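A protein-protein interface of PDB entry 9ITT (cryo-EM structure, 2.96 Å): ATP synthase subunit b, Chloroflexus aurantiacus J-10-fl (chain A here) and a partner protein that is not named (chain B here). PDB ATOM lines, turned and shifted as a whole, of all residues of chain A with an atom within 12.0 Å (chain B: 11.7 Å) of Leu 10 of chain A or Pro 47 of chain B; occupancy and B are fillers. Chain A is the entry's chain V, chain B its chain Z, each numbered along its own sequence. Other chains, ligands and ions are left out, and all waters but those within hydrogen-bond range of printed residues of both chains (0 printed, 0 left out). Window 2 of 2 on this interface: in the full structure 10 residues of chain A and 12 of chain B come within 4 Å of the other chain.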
ATOM      1  N   GLY A   5     -20.313  -8.289  15.398  1.00  0.00           N
ATOM      2  CA  GLY A   5     -20.940  -9.336  14.612  1.00  0.00           C
ATOM      3  C   GLY A   5     -22.281  -9.768  15.175  1.00  0.00           C
ATOM      4  O   GLY A   5     -22.395 -10.087  16.358  1.00  0.00           O
ATOM      5  N   ILE A   6     -23.297  -9.780  14.320  1.00  0.00           N
ATOM      6  CA  ILE A   6     -24.643 -10.158  14.736  1.00  0.00           C
ATOM      7  C   ILE A   6     -24.747 -11.676  14.761  1.00  0.00           C
ATOM      8  O   ILE A   6     -24.448 -12.349  13.768  1.00  0.00           O
ATOM      9  CB  ILE A   6     -25.696  -9.541  13.802  1.00  0.00           C
ATOM     10  CG1 ILE A   6     -25.664  -8.007  13.898  1.00  0.00           C
ATOM     11  CG2 ILE A   6     -27.085 -10.102  14.124  1.00  0.00           C
ATOM     12  CD1 ILE A   6     -24.698  -7.339  12.934  1.00  0.00           C
ATOM     13  N   ASN A   7     -25.179 -12.217  15.899  1.00  0.00           N
ATOM     14  CA  ASN A   7     -25.325 -13.653  16.111  1.00  0.00           C
ATOM     15  C   ASN A   7     -26.804 -14.045  16.063  1.00  0.00           C
ATOM     16  O   ASN A   7     -27.611 -13.488  16.814  1.00  0.00           O
ATOM     17  CB  ASN A   7     -24.736 -14.055  17.459  1.00  0.00           C
ATOM     18  CG  ASN A   7     -24.549 -15.553  17.591  1.00  0.00           C
ATOM     19  OD1 ASN A   7     -24.837 -16.312  16.667  1.00  0.00           O
ATOM     20  ND2 ASN A   7     -24.065 -15.987  18.749  1.00  0.00           N
ATOM     21  N   PRO A   8     -27.225 -14.977  15.195  1.00  0.00           N
ATOM     22  CA  PRO A   8     -28.647 -15.366  15.198  1.00  0.00           C
ATOM     23  C   PRO A   8     -29.126 -15.909  16.533  1.00  0.00           C
ATOM     24  O   PRO A   8     -30.289 -15.689  16.893  1.00  0.00           O
ATOM     25  CB  PRO A   8     -28.724 -16.434  14.098  1.00  0.00           C
ATOM     26  CG  PRO A   8     -27.581 -16.141  13.206  1.00  0.00           C
ATOM     27  CD  PRO A   8     -26.492 -15.639  14.100  1.00  0.00           C
ATOM     28  N   THR A   9     -28.275 -16.621  17.277  1.00  0.00           N
ATOM     29  CA  THR A   9     -28.680 -17.093  18.596  1.00  0.00           C
ATOM     30  C   THR A   9     -28.965 -15.925  19.530  1.00  0.00           C
ATOM     31  O   THR A   9     -29.965 -15.933  20.255  1.00  0.00           O
ATOM     32  CB  THR A   9     -27.601 -18.002  19.188  1.00  0.00           C
ATOM     33  OG1 THR A   9     -26.329 -17.350  19.119  1.00  0.00           O
ATOM     34  CG2 THR A   9     -27.537 -19.316  18.426  1.00  0.00           C
ATOM     35  N   LEU A  10     -28.106 -14.901  19.518  1.00  0.00           N
ATOM     36  CA  LEU A  10     -28.375 -13.712  20.319  1.00  0.00           C
ATOM     37  C   LEU A  10     -29.609 -12.972  19.826  1.00  0.00           C
ATOM     38  O   LEU A  10     -30.336 -12.382  20.629  1.00  0.00           O
ATOM     39  CB  LEU A  10     -27.164 -12.781  20.309  1.00  0.00           C
ATOM     40  CG  LEU A  10     -25.895 -13.333  20.960  1.00  0.00           C
ATOM     41  CD1 LEU A  10     -24.709 -12.413  20.703  1.00  0.00           C
ATOM     42  CD2 LEU A  10     -26.110 -13.532  22.455  1.00  0.00           C
ATOM     43  N   PHE A  11     -29.860 -12.986  18.517  1.00  0.00           N
ATOM     44  CA  PHE A  11     -31.071 -12.371  17.981  1.00  0.00           C
ATOM     45  C   PHE A  11     -32.314 -13.058  18.540  1.00  0.00           C
ATOM     46  O   PHE A  11     -33.245 -12.401  19.031  1.00  0.00           O
ATOM     47  CB  PHE A  11     -31.029 -12.452  16.454  1.00  0.00           C
ATOM     48  CG  PHE A  11     -32.224 -11.863  15.769  1.00  0.00           C
ATOM     49  CD1 PHE A  11     -32.599 -10.554  16.004  1.00  0.00           C
ATOM     50  CD2 PHE A  11     -32.965 -12.618  14.875  1.00  0.00           C
ATOM     51  CE1 PHE A  11     -33.691 -10.011  15.366  1.00  0.00           C
ATOM     52  CE2 PHE A  11     -34.062 -12.077  14.235  1.00  0.00           C
ATOM     53  CZ  PHE A  11     -34.425 -10.772  14.480  1.00  0.00           C
ATOM     54  N   ILE A  12     -32.327 -14.391  18.510  1.00  0.00           N
ATOM     55  CA  ILE A  12     -33.446 -15.132  19.079  1.00  0.00           C
ATOM     56  C   ILE A  12     -33.532 -14.888  20.580  1.00  0.00           C
ATOM     57  O   ILE A  12     -34.625 -14.847  21.151  1.00  0.00           O
ATOM     58  CB  ILE A  12     -33.324 -16.631  18.745  1.00  0.00           C
ATOM     59  CG1 ILE A  12     -33.510 -16.847  17.238  1.00  0.00           C
ATOM     60  CG2 ILE A  12     -34.352 -17.434  19.549  1.00  0.00           C
ATOM     61  CD1 ILE A  12     -33.179 -18.248  16.753  1.00  0.00           C
ATOM     62  N   ALA A  13     -32.387 -14.728  21.246  1.00  0.00           N
ATOM     63  CA  ALA A  13     -32.390 -14.377  22.660  1.00  0.00           C
ATOM     64  C   ALA A  13     -33.042 -13.026  22.920  1.00  0.00           C
ATOM     65  O   ALA A  13     -33.752 -12.877  23.920  1.00  0.00           O
ATOM     66  CB  ALA A  13     -30.962 -14.375  23.210  1.00  0.00           C
ATOM     67  N   GLN A  14     -32.807 -12.037  22.055  1.00  0.00           N
ATOM     68  CA  GLN A  14     -33.547 -10.784  22.166  1.00  0.00           C
ATOM     69  C   GLN A  14     -35.038 -11.027  21.990  1.00  0.00           C
ATOM     70  O   GLN A  14     -35.861 -10.395  22.666  1.00  0.00           O
ATOM     71  CB  GLN A  14     -33.072  -9.757  21.135  1.00  0.00           C
ATOM     72  CG  GLN A  14     -31.585  -9.436  21.133  1.00  0.00           C
ATOM     73  CD  GLN A  14     -31.014  -9.205  22.514  1.00  0.00           C
ATOM     74  OE1 GLN A  14     -31.377  -8.248  23.198  1.00  0.00           O
ATOM     75  NE2 GLN A  14     -30.106 -10.080  22.928  1.00  0.00           N
ATOM     76  N   LEU A  15     -35.408 -11.927  21.073  1.00  0.00           N
ATOM     77  CA  LEU A  15     -36.826 -12.263  20.937  1.00  0.00           C
ATOM     78  C   LEU A  15     -37.392 -12.857  22.224  1.00  0.00           C
ATOM     79  O   LEU A  15     -38.511 -12.514  22.617  1.00  0.00           O
ATOM     80  CB  LEU A  15     -37.064 -13.230  19.772  1.00  0.00           C
ATOM     81  CG  LEU A  15     -36.506 -12.886  18.390  1.00  0.00           C
ATOM     82  CD1 LEU A  15     -36.696 -14.058  17.438  1.00  0.00           C
ATOM     83  CD2 LEU A  15     -37.173 -11.640  17.827  1.00  0.00           C
ATOM     84  N   ILE A  16     -36.649 -13.744  22.891  1.00  0.00           N
ATOM     85  CA  ILE A  16     -37.140 -14.314  24.148  1.00  0.00           C
ATOM     86  C   ILE A  16     -37.226 -13.240  25.228  1.00  0.00           C
ATOM     87  O   ILE A  16     -38.159 -13.234  26.042  1.00  0.00           O
ATOM     88  CB  ILE A  16     -36.269 -15.500  24.615  1.00  0.00           C
ATOM     89  CG1 ILE A  16     -36.073 -16.542  23.506  1.00  0.00           C
ATOM     90  CG2 ILE A  16     -36.881 -16.156  25.854  1.00  0.00           C
ATOM     91  CD1 ILE A  16     -37.343 -16.959  22.787  1.00  0.00           C
ATOM     92  N   ASN A  17     -36.246 -12.335  25.276  1.00  0.00           N
ATOM     93  CA  ASN A  17     -36.311 -11.240  26.240  1.00  0.00           C
ATOM     94  C   ASN A  17     -37.558 -10.399  26.018  1.00  0.00           C
ATOM     95  O   ASN A  17     -38.274 -10.072  26.972  1.00  0.00           O
ATOM     96  CB  ASN A  17     -35.060 -10.364  26.146  1.00  0.00           C
ATOM     97  CG  ASN A  17     -34.939  -9.386  27.311  1.00  0.00           C
ATOM     98  OD1 ASN A  17     -35.930  -8.829  27.782  1.00  0.00           O
ATOM     99  ND2 ASN A  17     -33.714  -9.165  27.770  1.00  0.00           N
ATOM    100  N   PHE A  18     -37.843 -10.049  24.764  1.00  0.00           N
ATOM    101  CA  PHE A  18     -39.024  -9.240  24.496  1.00  0.00           C
ATOM    102  C   PHE A  18     -40.306 -10.038  24.695  1.00  0.00           C
ATOM    103  O   PHE A  18     -41.349  -9.452  24.985  1.00  0.00           O
ATOM    104  CB  PHE A  18     -38.969  -8.658  23.085  1.00  0.00           C
ATOM    105  CG  PHE A  18     -39.746  -7.380  22.933  1.00  0.00           C
ATOM    106  CD1 PHE A  18     -39.281  -6.200  23.492  1.00  0.00           C
ATOM    107  CD2 PHE A  18     -40.942  -7.357  22.235  1.00  0.00           C
ATOM    108  CE1 PHE A  18     -39.995  -5.023  23.359  1.00  0.00           C
ATOM    109  CE2 PHE A  18     -41.658  -6.183  22.097  1.00  0.00           C
ATOM    110  CZ  PHE A  18     -41.183  -5.015  22.659  1.00  0.00           C
ATOM    111  N   LEU A  19     -40.251 -11.364  24.559  1.00  0.00           N
ATOM    112  CA  LEU A  19     -41.416 -12.187  24.871  1.00  0.00           C
ATOM    113  C   LEU A  19     -41.724 -12.141  26.363  1.00  0.00           C
ATOM    114  O   LEU A  19     -42.874 -11.928  26.767  1.00  0.00           O
ATOM    115  CB  LEU A  19     -41.175 -13.629  24.418  1.00  0.00           C
ATOM    116  CG  LEU A  19     -41.479 -13.989  22.960  1.00  0.00           C
ATOM    117  CD1 LEU A  19     -41.124 -15.444  22.704  1.00  0.00           C
ATOM    118  CD2 LEU A  19     -42.938 -13.732  22.603  1.00  0.00           C
ATOM    119  N   GLU B  37     -21.304  -2.026  18.792  1.00  0.00           N
ATOM    120  CA  GLU B  37     -21.828  -3.116  19.602  1.00  0.00           C
ATOM    121  C   GLU B  37     -20.746  -3.589  20.559  1.00  0.00           C
ATOM    122  O   GLU B  37     -19.573  -3.679  20.185  1.00  0.00           O
ATOM    123  CB  GLU B  37     -22.301  -4.291  18.733  1.00  0.00           C
ATOM    124  N   VAL B  38     -21.147  -3.888  21.797  1.00  0.00           N
ATOM    125  CA  VAL B  38     -20.241  -4.393  22.819  1.00  0.00           C
ATOM    126  C   VAL B  38     -20.911  -5.554  23.540  1.00  0.00           C
ATOM    127  O   VAL B  38     -22.138  -5.669  23.580  1.00  0.00           O
ATOM    128  CB  VAL B  38     -19.824  -3.297  23.826  1.00  0.00           C
ATOM    129  N   ILE B  39     -20.079  -6.418  24.121  1.00  0.00           N
ATOM    130  CA  ILE B  39     -20.522  -7.652  24.759  1.00  0.00           C
ATOM    131  C   ILE B  39     -20.008  -7.666  26.192  1.00  0.00           C
ATOM    132  O   ILE B  39     -18.830  -7.383  26.438  1.00  0.00           O
ATOM    133  CB  ILE B  39     -20.034  -8.897  23.989  1.00  0.00           C
ATOM    134  N   PHE B  40     -20.895  -7.997  27.131  1.00  0.00           N
ATOM    135  CA  PHE B  40     -20.550  -8.108  28.542  1.00  0.00           C
ATOM    136  C   PHE B  40     -20.339  -9.553  28.971  1.00  0.00           C
ATOM    137  O   PHE B  40     -19.502  -9.817  29.842  1.00  0.00           O
ATOM    138  CB  PHE B  40     -21.648  -7.468  29.396  1.00  0.00           C
ATOM    139  N   ASP B  41     -21.073 -10.489  28.373  1.00  0.00           N
ATOM    140  CA  ASP B  41     -20.944 -11.923  28.661  1.00  0.00           C
ATOM    141  C   ASP B  41     -21.267 -12.126  30.141  1.00  0.00           C
ATOM    142  O   ASP B  41     -22.338 -11.682  30.588  1.00  0.00           O
ATOM    143  CB  ASP B  41     -19.566 -12.392  28.207  1.00  0.00           C
ATOM    144  N   GLY B  42     -20.403 -12.775  30.925  1.00  0.00           N
ATOM    145  CA  GLY B  42     -20.632 -13.005  32.333  1.00  0.00           C
ATOM    146  C   GLY B  42     -21.163 -14.384  32.670  1.00  0.00           C
ATOM    147  O   GLY B  42     -21.101 -14.784  33.838  1.00  0.00           O
ATOM    148  N   ILE B  43     -21.682 -15.113  31.686  1.00  0.00           N
ATOM    149  CA  ILE B  43     -22.194 -16.466  31.898  1.00  0.00           C
ATOM    150  C   ILE B  43     -21.738 -17.359  30.747  1.00  0.00           C
ATOM    151  O   ILE B  43     -21.492 -16.855  29.641  1.00  0.00           O
ATOM    152  CB  ILE B  43     -23.726 -16.469  32.030  1.00  0.00           C
ATOM    153  N   PRO B  44     -21.609 -18.671  30.944  1.00  0.00           N
ATOM    154  CA  PRO B  44     -21.327 -19.550  29.806  1.00  0.00           C
ATOM    155  C   PRO B  44     -22.527 -19.646  28.876  1.00  0.00           C
ATOM    156  O   PRO B  44     -23.675 -19.448  29.282  1.00  0.00           O
ATOM    157  CB  PRO B  44     -21.019 -20.899  30.464  1.00  0.00           C
ATOM    158  N   GLY B  45     -22.246 -19.949  27.612  1.00  0.00           N
ATOM    159  CA  GLY B  45     -23.300 -20.095  26.628  1.00  0.00           C
ATOM    160  C   GLY B  45     -23.641 -18.797  25.926  1.00  0.00           C
ATOM    161  O   GLY B  45     -22.987 -18.423  24.948  1.00  0.00           O
ATOM    162  N   PHE B  46     -24.671 -18.110  26.410  1.00  0.00           N
ATOM    163  CA  PHE B  46     -25.145 -16.893  25.761  1.00  0.00           C
ATOM    164  C   PHE B  46     -24.304 -15.699  26.205  1.00  0.00           C
ATOM    165  O   PHE B  46     -24.296 -15.377  27.399  1.00  0.00           O
ATOM    166  CB  PHE B  46     -26.610 -16.649  26.102  1.00  0.00           C
ATOM    167  N   PRO B  47     -23.584 -15.013  25.293  1.00  0.00           N
ATOM    168  CA  PRO B  47     -22.868 -13.784  25.719  1.00  0.00           C
ATOM    169  C   PRO B  47     -23.793 -12.579  25.889  1.00  0.00           C
ATOM    170  O   PRO B  47     -24.022 -11.776  24.983  1.00  0.00           O
ATOM    171  CB  PRO B  47     -21.853 -13.574  24.592  1.00  0.00           C
ATOM    172  N   ILE B  48     -24.365 -12.464  27.090  1.00  0.00           N
ATOM    173  CA  ILE B  48     -25.251 -11.347  27.397  1.00  0.00           C
ATOM    174  C   ILE B  48     -24.508 -10.027  27.225  1.00  0.00           C
ATOM    175  O   ILE B  48     -23.360  -9.872  27.662  1.00  0.00           O
ATOM    176  CB  ILE B  48     -25.813 -11.499  28.822  1.00  0.00           C
ATOM    177  N   THR B  49     -25.170  -9.067  26.584  1.00  0.00           N
ATOM    178  CA  THR B  49     -24.606  -7.757  26.294  1.00  0.00           C
ATOM    179  C   THR B  49     -25.070  -6.739  27.329  1.00  0.00           C
ATOM    180  O   THR B  49     -26.007  -6.978  28.094  1.00  0.00           O
ATOM    181  CB  THR B  49     -25.005  -7.280  24.891  1.00  0.00           C
ATOM    182  N   ASN B  50     -24.390  -5.589  27.350  1.00  0.00           N
ATOM    183  CA  ASN B  50     -24.807  -4.512  28.242  1.00  0.00           C
ATOM    184  C   ASN B  50     -26.134  -3.914  27.790  1.00  0.00           C
ATOM    185  O   ASN B  50     -26.954  -3.503  28.619  1.00  0.00           O
ATOM    186  CB  ASN B  50     -23.723  -3.436  28.317  1.00  0.00           C
ATOM    187  N   SER B  51     -26.361  -3.854  26.475  1.00  0.00           N
ATOM    188  CA  SER B  51     -27.668  -3.443  25.972  1.00  0.00           C
ATOM    189  C   SER B  51     -28.751  -4.403  26.442  1.00  0.00           C
ATOM    190  O   SER B  51     -29.861  -3.983  26.788  1.00  0.00           O
ATOM    191  CB  SER B  51     -27.641  -3.371  24.446  1.00  0.00           C
ATOM    192  N   PHE B  52     -28.442  -5.700  26.461  1.00  0.00           N
ATOM    193  CA  PHE B  52     -29.345  -6.679  27.054  1.00  0.00           C
ATOM    194  C   PHE B  52     -29.603  -6.373  28.525  1.00  0.00           C
ATOM    195  O   PHE B  52     -30.733  -6.525  29.006  1.00  0.00           O
ATOM    196  CB  PHE B  52     -28.740  -8.073  26.893  1.00  0.00           C
ATOM    197  N   VAL B  53     -28.573  -5.934  29.251  1.00  0.00           N
ATOM    198  CA  VAL B  53     -28.739  -5.613  30.666  1.00  0.00           C
ATOM    199  C   VAL B  53     -29.668  -4.417  30.835  1.00  0.00           C
ATOM    200  O   VAL B  53     -30.504  -4.387  31.745  1.00  0.00           O
ATOM    201  CB  VAL B  53     -27.367  -5.366  31.322  1.00  0.00           C
ATOM    202  N   VAL B  54     -29.524  -3.402  29.978  1.00  0.00           N
ATOM    203  CA  VAL B  54     -30.419  -2.251  30.058  1.00  0.00           C
ATOM    204  C   VAL B  54     -31.835  -2.656  29.674  1.00  0.00           C
ATOM    205  O   VAL B  54     -32.813  -2.147  30.230  1.00  0.00           O
ATOM    206  CB  VAL B  54     -29.903  -1.095  29.182  1.00  0.00           C
ATOM    207  N   ALA B  55     -31.972  -3.571  28.714  1.00  0.00           N
ATOM    208  CA  ALA B  55     -33.295  -4.090  28.395  1.00  0.00           C
ATOM    209  C   ALA B  55     -33.921  -4.750  29.617  1.00  0.00           C
ATOM    210  O   ALA B  55     -35.092  -4.509  29.932  1.00  0.00           O
ATOM    211  CB  ALA B  55     -33.205  -5.081  27.235  1.00  0.00           C
ATOM    212  N   PRO B 182     -17.814  -0.183  27.760  1.00  0.00           N
ATOM    213  CA  PRO B 182     -18.810   0.557  28.541  1.00  0.00           C
ATOM    214  C   PRO B 182     -20.017  -0.302  28.882  1.00  0.00           C
ATOM    215  O   PRO B 182     -20.396  -1.212  28.140  1.00  0.00           O
ATOM    216  CB  PRO B 182     -19.195   1.718  27.622  1.00  0.00           C
ATOM    217  N   PRO B 187     -30.957  -0.043  24.751  1.00  0.00           N
ATOM    218  CA  PRO B 187     -31.366  -1.234  23.986  1.00  0.00           C
ATOM    219  C   PRO B 187     -31.540  -0.955  22.506  1.00  0.00           C
ATOM    220  O   PRO B 187     -31.277  -1.834  21.674  1.00  0.00           O
ATOM    221  CB  PRO B 187     -32.687  -1.640  24.652  1.00  0.00           C
ATOM    222  N   ASP B 190     -28.544  -1.353  20.077  1.00  0.00           N
ATOM    223  CA  ASP B 190     -28.207  -2.685  19.596  1.00  0.00           C
ATOM    224  C   ASP B 190     -29.113  -3.041  18.426  1.00  0.00           C
ATOM    225  O   ASP B 190     -30.341  -2.957  18.538  1.00  0.00           O
ATOM    226  CB  ASP B 190     -28.354  -3.718  20.713  1.00  0.00           C
ATOM    227  N   LEU B 191     -28.505  -3.436  17.306  1.00  0.00           N
ATOM    228  CA  LEU B 191     -29.287  -3.877  16.157  1.00  0.00           C
ATOM    229  C   LEU B 191     -30.093  -5.127  16.488  1.00  0.00           C
ATOM    230  O   LEU B 191     -31.180  -5.337  15.939  1.00  0.00           O
ATOM    231  CB  LEU B 191     -28.367  -4.138  14.965  1.00  0.00           C
ATOM    232  N   ASN B 192     -29.572  -5.970  17.384  1.00  0.00           N
ATOM    233  CA  ASN B 192     -30.248  -7.215  17.729  1.00  0.00           C
ATOM    234  C   ASN B 192     -31.639  -6.978  18.303  1.00  0.00           C
ATOM    235  O   ASN B 192     -32.516  -7.834  18.147  1.00  0.00           O
ATOM    236  CB  ASN B 192     -29.399  -8.003  18.731  1.00  0.00           C
ATOM    237  N   PHE B 193     -31.859  -5.840  18.962  1.00  0.00           N
ATOM    238  CA  PHE B 193     -33.159  -5.505  19.531  1.00  0.00           C
ATOM    239  C   PHE B 193     -34.077  -4.839  18.512  1.00  0.00           C
ATOM    240  O   PHE B 193     -35.258  -5.193  18.410  1.00  0.00           O
ATOM    241  CB  PHE B 193     -32.975  -4.588  20.744  1.00  0.00           C
ATOM    242  N   THR B 194     -33.559  -3.857  17.771  1.00  0.00           N
ATOM    243  CA  THR B 194     -34.388  -3.164  16.791  1.00  0.00           C
ATOM    244  C   THR B 194     -34.864  -4.118  15.704  1.00  0.00           C
ATOM    245  O   THR B 194     -36.034  -4.082  15.304  1.00  0.00           O
ATOM    246  CB  THR B 194     -33.615  -1.996  16.177  1.00  0.00           C
ATOM    247  N   PHE B 195     -33.974  -4.990  15.221  1.00  0.00           N
ATOM    248  CA  PHE B 195     -34.388  -5.986  14.239  1.00  0.00           C
ATOM    249  C   PHE B 195     -35.399  -6.954  14.839  1.00  0.00           C
ATOM    250  O   PHE B 195     -36.296  -7.431  14.138  1.00  0.00           O
ATOM    251  CB  PHE B 195     -33.173  -6.743  13.707  1.00  0.00           C
ATOM    252  N   ALA B 196     -35.268  -7.257  16.132  1.00  0.00           N
ATOM    253  CA  ALA B 196     -36.237  -8.135  16.780  1.00  0.00           C
ATOM    254  C   ALA B 196     -37.626  -7.509  16.782  1.00  0.00           C
ATOM    255  O   ALA B 196     -38.616  -8.165  16.436  1.00  0.00           O
ATOM    256  CB  ALA B 196     -35.786  -8.449  18.207  1.00  0.00           C
ATOM    257  N   ILE B 197     -37.715  -6.233  17.159  1.00  0.00           N
ATOM    258  CA  ILE B 197     -39.012  -5.559  17.146  1.00  0.00           C
ATOM    259  C   ILE B 197     -39.545  -5.475  15.721  1.00  0.00           C
ATOM    260  O   ILE B 197     -40.743  -5.668  15.479  1.00  0.00           O
ATOM    261  CB  ILE B 197     -38.919  -4.165  17.796  1.00  0.00           C
ATOM    262  N   VAL B 199     -38.972  -7.478  13.100  1.00  0.00           N
ATOM    263  CA  VAL B 199     -39.453  -8.763  12.602  1.00  0.00           C
ATOM    264  C   VAL B 199     -40.712  -9.192  13.344  1.00  0.00           C
ATOM    265  O   VAL B 199     -41.599  -9.818  12.754  1.00  0.00           O
ATOM    266  CB  VAL B 199     -38.341  -9.831  12.674  1.00  0.00           C
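NE2 of Gln 14 of chain A lies close to O of Leu 10 of chain A, 3.3 Å away.
Of the 30 printed residues of chain B, 4 touch a printed residue of chain A. Hydrophobic or aromatic side chains of chain B that line the printed part of chain A: Phe 195 and Ala 196. Of the 15 printed residues of chain A, 4 touch a printed residue of chain B. Printed residues of chain A that touch a printed residue of chain B: Leu 10, Phe 11, Gln 14 and Leu 15. Hydrophobic or aromatic side chains of chain A that line the printed part of chain B: Leu 10, Phe 11 and Leu 15. Among the printed residues, 6 pairs touch across the chains. Among the printed residues, no Asp or Glu carboxylate lies within 4 Å of a Lys or Arg side-chain nitrogen of the other chain.
Among the printed residues, pairs that only touch across the chains: Phe 11 of chain A with Ala 196 of chain B, Phe 11 of chain A with Asn 192 of chain B, Leu 15 of chain A with Ala 196 of chain B, Gln 14 of chain A with Asn 192 of chain B, Phe 11 of chain A with Phe 195 of chain B and Leu 10 of chain A with Pro 47 of chain B.
No residue of chain B comes within 4 Å of Asn 7 of chain A. No residue of chain B comes within 4 Å of Pro 8 of chain A. Of chain B, only Pro 47 (3.7 Å) comes within 4 Å of Leu 10 of chain A. No residue of chain B comes within 4 Å of Ile 12 of chain A. Of the printed residues of chain B, Gln 14 of chain A touches Asn 192 (3.5 Å). Printed residues of chain B within 4 Å of Leu 15 of chain A: Ala 196. Val 38 of chain B touches none of the printed residues of chain A. No residue of chain A comes within 4 Å of Asp 41 of chain B. No residue of chain A comes within 4 Å of Ile 43 of chain B. Pro 44 of chain B touches none of the printed residues of chain A. No residue of chain A comes within 4 Å of Thr 49 of chain B. Asn 192 of chain B touches two residues of chain A. Printed residues of chain A within 4 Å of Ala 196 of chain B: Phe 11 (3.3 Å) and Leu 15 (3.5 Å). The nearest residue of chain B that does not touch Leu 10 of chain A is Phe 46 of chain B (4.7 Å).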
